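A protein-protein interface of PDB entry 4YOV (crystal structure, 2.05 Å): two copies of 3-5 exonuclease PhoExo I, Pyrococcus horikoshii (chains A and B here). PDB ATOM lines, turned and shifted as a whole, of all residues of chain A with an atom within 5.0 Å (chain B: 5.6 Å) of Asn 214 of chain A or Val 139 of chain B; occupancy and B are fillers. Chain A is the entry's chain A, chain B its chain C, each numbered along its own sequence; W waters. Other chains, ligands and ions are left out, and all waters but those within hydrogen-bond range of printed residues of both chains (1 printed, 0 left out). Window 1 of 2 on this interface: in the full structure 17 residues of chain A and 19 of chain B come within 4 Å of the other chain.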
ATOM      1  N   LEU A  13     -29.117 -20.439  26.363  1.00  0.00           N
ATOM      2  CA  LEU A  13     -28.462 -20.535  25.063  1.00  0.00           C
ATOM      3  C   LEU A  13     -28.182 -22.004  24.737  1.00  0.00           C
ATOM      4  O   LEU A  13     -28.003 -22.815  25.649  1.00  0.00           O
ATOM      5  CB  LEU A  13     -27.171 -19.721  25.043  1.00  0.00           C
ATOM      6  CG  LEU A  13     -27.190 -18.262  25.521  1.00  0.00           C
ATOM      7  CD1 LEU A  13     -25.791 -17.666  25.372  1.00  0.00           C
ATOM      8  CD2 LEU A  13     -28.216 -17.449  24.761  1.00  0.00           C
ATOM      9  N   PHE A  17     -24.445 -21.049  21.102  1.00  0.00           N
ATOM     10  CA  PHE A  17     -24.752 -19.729  21.672  1.00  0.00           C
ATOM     11  C   PHE A  17     -26.005 -19.061  21.072  1.00  0.00           C
ATOM     12  O   PHE A  17     -26.183 -17.860  21.186  1.00  0.00           O
ATOM     13  CB  PHE A  17     -23.524 -18.794  21.542  1.00  0.00           C
ATOM     14  CG  PHE A  17     -22.289 -19.342  22.202  1.00  0.00           C
ATOM     15  CD1 PHE A  17     -22.165 -19.354  23.578  1.00  0.00           C
ATOM     16  CD2 PHE A  17     -21.259 -19.862  21.444  1.00  0.00           C
ATOM     17  CE1 PHE A  17     -21.032 -19.879  24.183  1.00  0.00           C
ATOM     18  CE2 PHE A  17     -20.130 -20.393  22.043  1.00  0.00           C
ATOM     19  CZ  PHE A  17     -20.020 -20.403  23.413  1.00  0.00           C
ATOM     20  N   TYR A 212     -17.892 -15.808  30.945  1.00  0.00           N
ATOM     21  CA  TYR A 212     -16.960 -15.478  29.870  1.00  0.00           C
ATOM     22  C   TYR A 212     -17.708 -14.770  28.739  1.00  0.00           C
ATOM     23  O   TYR A 212     -18.943 -14.769  28.720  1.00  0.00           O
ATOM     24  CB  TYR A 212     -16.228 -16.754  29.357  1.00  0.00           C
ATOM     25  CG  TYR A 212     -17.128 -17.861  28.867  1.00  0.00           C
ATOM     26  CD1 TYR A 212     -17.630 -17.852  27.571  1.00  0.00           C
ATOM     27  CD2 TYR A 212     -17.438 -18.935  29.685  1.00  0.00           C
ATOM     28  CE1 TYR A 212     -18.439 -18.883  27.110  1.00  0.00           C
ATOM     29  CE2 TYR A 212     -18.255 -19.967  29.237  1.00  0.00           C
ATOM     30  CZ  TYR A 212     -18.753 -19.925  27.949  1.00  0.00           C
ATOM     31  OH  TYR A 212     -19.555 -20.936  27.506  1.00  0.00           O
ATOM     32  N   PRO A 213     -16.968 -14.129  27.825  1.00  0.00           N
ATOM     33  CA  PRO A 213     -17.578 -13.458  26.675  1.00  0.00           C
ATOM     34  C   PRO A 213     -18.282 -14.427  25.708  1.00  0.00           C
ATOM     35  O   PRO A 213     -17.721 -15.467  25.313  1.00  0.00           O
ATOM     36  CB  PRO A 213     -16.378 -12.819  25.961  1.00  0.00           C
ATOM     37  CG  PRO A 213     -15.340 -12.680  27.009  1.00  0.00           C
ATOM     38  CD  PRO A 213     -15.508 -13.882  27.886  1.00  0.00           C
ATOM     39  N   ASN A 214     -19.499 -14.058  25.325  1.00  0.00           N
ATOM     40  CA  ASN A 214     -20.187 -14.648  24.188  1.00  0.00           C
ATOM     41  C   ASN A 214     -19.423 -14.357  22.918  1.00  0.00           C
ATOM     42  O   ASN A 214     -19.358 -13.210  22.491  1.00  0.00           O
ATOM     43  CB  ASN A 214     -21.615 -14.097  24.092  1.00  0.00           C
ATOM     44  CG  ASN A 214     -22.451 -14.796  23.012  1.00  0.00           C
ATOM     45  OD1 ASN A 214     -21.936 -15.246  21.987  1.00  0.00           O
ATOM     46  ND2 ASN A 214     -23.743 -14.884  23.256  1.00  0.00           N
ATOM     47  N   PRO A 215     -18.890 -15.409  22.261  1.00  0.00           N
ATOM     48  CA  PRO A 215     -18.028 -15.132  21.110  1.00  0.00           C
ATOM     49  C   PRO A 215     -18.741 -14.536  19.909  1.00  0.00           C
ATOM     50  O   PRO A 215     -18.087 -13.936  19.048  1.00  0.00           O
ATOM     51  CB  PRO A 215     -17.412 -16.521  20.779  1.00  0.00           C
ATOM     52  CG  PRO A 215     -18.331 -17.512  21.381  1.00  0.00           C
ATOM     53  CD  PRO A 215     -18.903 -16.830  22.629  1.00  0.00           C
ATOM     54  N   LEU A 216     -20.056 -14.687  19.838  1.00  0.00           N
ATOM     55  CA  LEU A 216     -20.781 -14.249  18.653  1.00  0.00           C
ATOM     56  C   LEU A 216     -21.476 -12.914  18.861  1.00  0.00           C
ATOM     57  O   LEU A 216     -22.016 -12.327  17.915  1.00  0.00           O
ATOM     58  CB  LEU A 216     -21.834 -15.298  18.250  1.00  0.00           C
ATOM     59  CG  LEU A 216     -21.258 -16.703  18.063  1.00  0.00           C
ATOM     60  CD1 LEU A 216     -22.359 -17.631  17.497  1.00  0.00           C
ATOM     61  CD2 LEU A 216     -20.019 -16.654  17.173  1.00  0.00           C
ATOM     62  N   VAL A 217     -21.514 -12.467  20.107  1.00  0.00           N
ATOM     63  CA  VAL A 217     -22.202 -11.214  20.452  1.00  0.00           C
ATOM     64  C   VAL A 217     -21.323 -10.387  21.404  1.00  0.00           C
ATOM     65  O   VAL A 217     -21.439 -10.512  22.620  1.00  0.00           O
ATOM     66  CB  VAL A 217     -23.589 -11.484  21.112  1.00  0.00           C
ATOM     67  CG1 VAL A 217     -24.467 -10.241  21.026  1.00  0.00           C
ATOM     68  CG2 VAL A 217     -24.319 -12.686  20.440  1.00  0.00           C
ATOM     69  N   ARG A 218     -20.423  -9.578  20.839  1.00  0.00           N
ATOM     70  CA  ARG A 218     -19.466  -8.779  21.622  1.00  0.00           C
ATOM     71  C   ARG A 218     -20.177  -7.854  22.652  1.00  0.00           C
ATOM     72  O   ARG A 218     -21.200  -7.290  22.343  1.00  0.00           O
ATOM     73  CB  ARG A 218     -18.584  -7.961  20.673  1.00  0.00           C
ATOM     74  CG  ARG A 218     -17.420  -7.273  21.354  1.00  0.00           C
ATOM     75  CD  ARG A 218     -16.317  -6.863  20.398  1.00  0.00           C
ATOM     76  NE  ARG A 218     -16.722  -5.944  19.341  1.00  0.00           N
ATOM     77  CZ  ARG A 218     -16.190  -4.738  19.157  1.00  0.00           C
ATOM     78  NH1 ARG A 218     -16.610  -3.976  18.158  1.00  0.00           N
ATOM     79  NH2 ARG A 218     -15.244  -4.283  19.972  1.00  0.00           N
ATOM     80  N   PHE A 220     -21.557  -8.960  25.363  1.00  0.00           N
ATOM     81  CA  PHE A 220     -22.480  -9.769  26.172  1.00  0.00           C
ATOM     82  C   PHE A 220     -21.732 -10.949  26.823  1.00  0.00           C
ATOM     83  O   PHE A 220     -20.904 -11.582  26.182  1.00  0.00           O
ATOM     84  CB  PHE A 220     -23.659 -10.300  25.337  1.00  0.00           C
ATOM     85  CG  PHE A 220     -24.669  -9.246  24.931  1.00  0.00           C
ATOM     86  CD1 PHE A 220     -24.376  -8.323  23.947  1.00  0.00           C
ATOM     87  CD2 PHE A 220     -25.950  -9.259  25.474  1.00  0.00           C
ATOM     88  CE1 PHE A 220     -25.328  -7.421  23.513  1.00  0.00           C
ATOM     89  CE2 PHE A 220     -26.931  -8.331  25.068  1.00  0.00           C
ATOM     90  CZ  PHE A 220     -26.629  -7.415  24.084  1.00  0.00           C
ATOM     91  N   MET A 221     -22.003 -11.237  28.092  1.00  0.00           N
ATOM     92  CA  MET A 221     -21.315 -12.348  28.760  1.00  0.00           C
ATOM     93  C   MET A 221     -22.201 -13.595  28.822  1.00  0.00           C
ATOM     94  O   MET A 221     -23.437 -13.515  28.719  1.00  0.00           O
ATOM     95  CB  MET A 221     -20.888 -11.937  30.177  1.00  0.00           C
ATOM     96  CG  MET A 221     -19.979 -10.717  30.226  1.00  0.00           C
ATOM     97  SD  MET A 221     -18.381 -11.000  29.431  1.00  0.00           S
ATOM     98  CE  MET A 221     -18.513  -9.917  28.003  1.00  0.00           C
ATOM     99  N   VAL A 222     -21.550 -14.747  28.956  1.00  0.00           N
ATOM    100  CA  VAL A 222     -22.224 -16.002  29.192  1.00  0.00           C
ATOM    101  C   VAL A 222     -21.916 -16.484  30.602  1.00  0.00           C
ATOM    102  O   VAL A 222     -20.770 -16.384  31.074  1.00  0.00           O
ATOM    103  CB  VAL A 222     -21.800 -17.084  28.142  1.00  0.00           C
ATOM    104  CG1 VAL A 222     -22.379 -18.427  28.484  1.00  0.00           C
ATOM    105  CG2 VAL A 222     -22.208 -16.644  26.751  1.00  0.00           C
ATOM    106  N   VAL B  30      -9.373 -18.734  18.210  1.00  0.00           N
ATOM    107  CA  VAL B  30      -9.956 -18.420  19.505  1.00  0.00           C
ATOM    108  C   VAL B  30     -10.822 -19.583  19.992  1.00  0.00           C
ATOM    109  O   VAL B  30     -11.690 -20.100  19.259  1.00  0.00           O
ATOM    110  CB  VAL B  30     -10.777 -17.098  19.456  1.00  0.00           C
ATOM    111  CG1 VAL B  30     -11.398 -16.807  20.792  1.00  0.00           C
ATOM    112  CG2 VAL B  30      -9.904 -15.929  19.024  1.00  0.00           C
ATOM    113  N   TYR B  34     -12.698 -17.553  25.209  1.00  0.00           N
ATOM    114  CA  TYR B  34     -12.899 -16.531  24.183  1.00  0.00           C
ATOM    115  C   TYR B  34     -12.389 -15.145  24.615  1.00  0.00           C
ATOM    116  O   TYR B  34     -12.939 -14.133  24.199  1.00  0.00           O
ATOM    117  CB  TYR B  34     -14.403 -16.446  23.808  1.00  0.00           C
ATOM    118  CG  TYR B  34     -15.029 -17.823  23.597  1.00  0.00           C
ATOM    119  CD1 TYR B  34     -14.711 -18.596  22.471  1.00  0.00           C
ATOM    120  CD2 TYR B  34     -15.910 -18.354  24.523  1.00  0.00           C
ATOM    121  CE1 TYR B  34     -15.262 -19.848  22.279  1.00  0.00           C
ATOM    122  CE2 TYR B  34     -16.469 -19.620  24.341  1.00  0.00           C
ATOM    123  CZ  TYR B  34     -16.137 -20.359  23.210  1.00  0.00           C
ATOM    124  OH  TYR B  34     -16.700 -21.602  23.017  1.00  0.00           O
ATOM    125  N   LYS B  35     -11.307 -15.112  25.389  1.00  0.00           N
ATOM    126  CA  LYS B  35     -10.742 -13.852  25.851  1.00  0.00           C
ATOM    127  C   LYS B  35      -9.433 -13.549  25.146  1.00  0.00           C
ATOM    128  O   LYS B  35      -9.028 -12.389  25.069  1.00  0.00           O
ATOM    129  CB  LYS B  35     -10.527 -13.874  27.357  1.00  0.00           C
ATOM    130  CG  LYS B  35     -11.821 -13.883  28.185  1.00  0.00           C
ATOM    131  CD  LYS B  35     -11.469 -14.062  29.664  1.00  0.00           C
ATOM    132  CE  LYS B  35     -12.672 -14.046  30.546  1.00  0.00           C
ATOM    133  NZ  LYS B  35     -12.301 -14.080  31.980  1.00  0.00           N
ATOM    134  N   HIS B  78     -14.268 -16.137  10.833  1.00  0.00           N
ATOM    135  CA  HIS B  78     -14.851 -14.798  10.897  1.00  0.00           C
ATOM    136  C   HIS B  78     -13.943 -13.818  10.187  1.00  0.00           C
ATOM    137  O   HIS B  78     -12.769 -13.688  10.533  1.00  0.00           O
ATOM    138  CB  HIS B  78     -15.046 -14.348  12.346  1.00  0.00           C
ATOM    139  CG  HIS B  78     -16.190 -15.021  13.031  1.00  0.00           C
ATOM    140  ND1 HIS B  78     -16.536 -14.761  14.340  1.00  0.00           N
ATOM    141  CD2 HIS B  78     -17.056 -15.966  12.589  1.00  0.00           C
ATOM    142  CE1 HIS B  78     -17.576 -15.506  14.673  1.00  0.00           C
ATOM    143  NE2 HIS B  78     -17.905 -16.252  13.628  1.00  0.00           N
ATOM    144  N   SER B 137     -19.631  -7.626  15.546  1.00  0.00           N
ATOM    145  CA  SER B 137     -20.277  -8.548  16.470  1.00  0.00           C
ATOM    146  C   SER B 137     -19.348  -9.637  17.016  1.00  0.00           C
ATOM    147  O   SER B 137     -19.622 -10.243  18.053  1.00  0.00           O
ATOM    148  CB  SER B 137     -21.469  -9.212  15.756  1.00  0.00           C
ATOM    149  OG  SER B 137     -22.241  -9.979  16.654  1.00  0.00           O
ATOM    150  N   SER B 138     -18.271  -9.916  16.296  1.00  0.00           N
ATOM    151  CA  SER B 138     -17.413 -11.054  16.635  1.00  0.00           C
ATOM    152  C   SER B 138     -16.322 -10.699  17.671  1.00  0.00           C
ATOM    153  O   SER B 138     -15.473  -9.854  17.436  1.00  0.00           O
ATOM    154  CB  SER B 138     -16.753 -11.603  15.365  1.00  0.00           C
ATOM    155  OG  SER B 138     -15.751 -12.584  15.639  1.00  0.00           O
ATOM    156  N   VAL B 139     -16.316 -11.420  18.785  1.00  0.00           N
ATOM    157  CA  VAL B 139     -15.240 -11.325  19.744  1.00  0.00           C
ATOM    158  C   VAL B 139     -13.932 -11.835  19.108  1.00  0.00           C
ATOM    159  O   VAL B 139     -12.933 -11.127  19.158  1.00  0.00           O
ATOM    160  CB  VAL B 139     -15.569 -12.119  21.031  1.00  0.00           C
ATOM    161  CG1 VAL B 139     -14.310 -12.301  21.887  1.00  0.00           C
ATOM    162  CG2 VAL B 139     -16.703 -11.423  21.824  1.00  0.00           C
ATOM    163  N   PRO B 140     -13.951 -13.005  18.415  1.00  0.00           N
ATOM    164  CA  PRO B 140     -12.700 -13.358  17.729  1.00  0.00           C
ATOM    165  C   PRO B 140     -12.152 -12.287  16.791  1.00  0.00           C
ATOM    166  O   PRO B 140     -10.940 -12.120  16.758  1.00  0.00           O
ATOM    167  CB  PRO B 140     -13.074 -14.643  16.948  1.00  0.00           C
ATOM    168  CG  PRO B 140     -14.053 -15.301  17.839  1.00  0.00           C
ATOM    169  CD  PRO B 140     -14.890 -14.141  18.430  1.00  0.00           C
ATOM    170  N   VAL B 141     -12.985 -11.579  16.040  1.00  0.00           N
ATOM    171  CA  VAL B 141     -12.444 -10.508  15.210  1.00  0.00           C
ATOM    172  C   VAL B 141     -11.766  -9.417  16.099  1.00  0.00           C
ATOM    173  O   VAL B 141     -10.727  -8.851  15.738  1.00  0.00           O
ATOM    174  CB  VAL B 141     -13.523  -9.888  14.322  1.00  0.00           C
ATOM    175  CG1 VAL B 141     -13.048  -8.571  13.737  1.00  0.00           C
ATOM    176  CG2 VAL B 141     -13.904 -10.863  13.179  1.00  0.00           C
ATOM    177  N   ARG B 142     -12.347  -9.138  17.259  1.00  0.00           N
ATOM    178  CA  ARG B 142     -11.798  -8.101  18.139  1.00  0.00           C
ATOM    179  C   ARG B 142     -10.440  -8.541  18.715  1.00  0.00           C
ATOM    180  O   ARG B 142      -9.519  -7.733  18.871  1.00  0.00           O
ATOM    181  CB  ARG B 142     -12.772  -7.755  19.277  1.00  0.00           C
ATOM    182  CG  ARG B 142     -12.134  -6.810  20.391  1.00  0.00           C
ATOM    183  CD  ARG B 142     -11.692  -5.455  19.844  1.00  0.00           C
ATOM    184  NE  ARG B 142     -11.327  -4.516  20.938  1.00  0.00           N
ATOM    185  CZ  ARG B 142     -10.635  -3.394  20.760  1.00  0.00           C
ATOM    186  NH1 ARG B 142     -10.199  -3.082  19.547  1.00  0.00           N
ATOM    187  NH2 ARG B 142     -10.350  -2.589  21.807  1.00  0.00           N
ATOM    188  N   ILE B 143     -10.320  -9.833  19.001  1.00  0.00           N
ATOM    189  CA  ILE B 143      -9.076 -10.390  19.477  1.00  0.00           C
ATOM    190  C   ILE B 143      -8.028 -10.332  18.360  1.00  0.00           C
ATOM    191  O   ILE B 143      -6.861 -10.070  18.607  1.00  0.00           O
ATOM    192  CB  ILE B 143      -9.284 -11.825  20.018  1.00  0.00           C
ATOM    193  CG1 ILE B 143     -10.156 -11.750  21.287  1.00  0.00           C
ATOM    194  CG2 ILE B 143      -7.904 -12.522  20.296  1.00  0.00           C
ATOM    195  CD1 ILE B 143     -10.532 -13.121  21.865  1.00  0.00           C
ATOM    196  N   ALA B 144      -8.432 -10.559  17.120  1.00  0.00           N
ATOM    197  CA  ALA B 144      -7.472 -10.421  16.029  1.00  0.00           C
ATOM    198  C   ALA B 144      -6.963  -8.989  15.931  1.00  0.00           C
ATOM    199  O   ALA B 144      -5.812  -8.762  15.597  1.00  0.00           O
ATOM    200  CB  ALA B 144      -8.065 -10.851  14.717  1.00  0.00           C
ATOM    201  N   GLU B 192     -16.199  -5.410  27.204  1.00  0.00           N
ATOM    202  CA  GLU B 192     -15.852  -6.544  26.328  1.00  0.00           C
ATOM    203  C   GLU B 192     -15.452  -7.774  27.125  1.00  0.00           C
ATOM    204  O   GLU B 192     -15.308  -8.884  26.568  1.00  0.00           O
ATOM    205  CB  GLU B 192     -14.726  -6.154  25.359  1.00  0.00           C
ATOM    206  CG  GLU B 192     -15.163  -5.125  24.317  1.00  0.00           C
ATOM    207  CD  GLU B 192     -14.117  -4.861  23.242  1.00  0.00           C
ATOM    208  OE1 GLU B 192     -14.514  -4.433  22.128  1.00  0.00           O
ATOM    209  OE2 GLU B 192     -12.906  -5.066  23.499  1.00  0.00           O
ATOM    210  N   LEU B 195     -10.592  -8.775  27.127  1.00  0.00           N
ATOM    211  CA  LEU B 195      -9.944  -9.325  25.940  1.00  0.00           C
ATOM    212  C   LEU B 195      -8.485  -8.890  25.895  1.00  0.00           C
ATOM    213  O   LEU B 195      -8.192  -7.710  26.091  1.00  0.00           O
ATOM    214  CB  LEU B 195     -10.663  -8.867  24.676  1.00  0.00           C
ATOM    215  CG  LEU B 195     -12.172  -9.104  24.700  1.00  0.00           C
ATOM    216  CD1 LEU B 195     -12.831  -8.566  23.438  1.00  0.00           C
ATOM    217  CD2 LEU B 195     -12.460 -10.581  24.894  1.00  0.00           C
HETATM  218  O   HOH W   1     -15.377  -7.456  16.494  1.00  0.00           O
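Water W1 bridges the backbone carbonyl oxygen of Ser 138 of chain B (2.6 Å) and the guanidinium group of Arg 218 of chain A (3.5 Å).
The side-chain carboxylate of Glu 192 of chain B is in salt-bridge range of the guanidinium group of Arg 142 of chain B.
The side-chain hydroxyl (OG) of Ser 138 of chain B lies within hydrogen-bond range of the backbone NH (N) of Val 141 of chain B.
The side-chain amide oxygen (OD1) of Asn 214 of chain A lies within hydrogen-bond range of the backbone NH (N) of Leu 216 of chain A (2.9 Å).
O of Phe 220 of chain A is in hydrogen-bond range of N of Asn 214 of chain A, 3.0 Å away.
OG of Ser 138 of chain B lies within hydrogen-bond range of ND1 of His 78 of chain B (2.7 Å).
The side-chain amide oxygen (OD1) of Asn 214 of chain A lies within hydrogen-bond range of the backbone NH (N) of Val 217 of chain A, at 3.4 Å.
The backbone carbonyl oxygen (O) of Leu 216 of chain A lies within hydrogen-bond range of the side-chain hydroxyl (OG) of Ser 137 of chain B (2.7 Å).
The backbone NH (N) of Val 139 of chain B sits at hydrogen-bond distance from the backbone carbonyl oxygen (O) of Pro 215 of chain A, at 3.1 Å.
NE of Arg 218 of chain A lies within salt-bridge range of OE1 of Glu 192 of chain B, 3.9 Å away.
N of Arg 218 of chain A is in hydrogen-bond range of O of Ser 137 of chain B (3.0 Å).
Asn 214 of chain A touches just one residue of chain B: Val 139 (3.3 Å).
Of the printed residues of chain B, Arg 218 of chain A touches Ser 137 (3.0 Å), Val 139 (3.8 Å), Arg 142 (3.7 Å) and Glu 192 (2.3 Å).
Val 30 of chain B touches none of the printed residues of chain A.
Of the printed residues of chain A, His 78 of chain B touches Leu 216 (3.7 Å).
Printed residues of chain A within 4 Å of Ser 138 of chain B: Pro 215 (3.8 Å).
Val 139 of chain B touches just these residues of chain A: Asn 214, Pro 215 and Arg 218.
Val 141 of chain B touches none of the printed residues of chain A.
Of the printed residues of chain A, Arg 142 of chain B touches Arg 218 (3.7 Å).
The nearest residue of chain B that does not touch Asn 214 of chain A is Ser 137 of chain B (5.3 Å).
The nearest printed residue of chain A that does not touch Tyr 34 of chain B is Asn 214 of chain A (5.5 Å).
Among the printed residues, pairs that only touch across the chains: Pro 215 of chain A with Pro 140 of chain B, Asn 214 of chain A with Val 139 of chain B, Tyr 212 of chain A with Tyr 34 of chain B, Pro 213 of chain A with Tyr 34 of chain B, Phe 17 of chain A with Tyr 34 of chain B, Val 217 of chain A with Ser 137 of chain B, Met 221 of chain A with Glu 192 of chain B, Leu 216 of chain A with His 78 of chain B, Pro 213 of chain A with Lys 35 of chain B, Arg 218 of chain A with Arg 142 of chain B, Pro 215 of chain A with Tyr 34 of chain B, Pro 215 of chain A with Ser 138 of chain B, Pro 213 of chain A with Glu 192 of chain B and Arg 218 of chain A with Val 139 of chain B.
No position is printed for both chains.
Of the 18 pairs that touch across the chains among the printed residues, none has its exchanged pair printed and touching as well.
Of the 14 printed residues of chain B, 9 touch a printed residue of chain A.
Hydrophobic or aromatic side chains of chain B that line the printed part of chain A: Tyr 34, His 78, Val 139 and Pro 140.
Of the 12 printed residues of chain A, 9 touch a printed residue of chain B.
Among the printed residues, 18 pairs touch across the chains.
Among the printed residues, Asp or Glu carboxylates within 4 Å of a Lys or Arg side-chain nitrogen of the other chain: Arg 218 of chain A with Glu 192 of chain B (2.3 Å).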
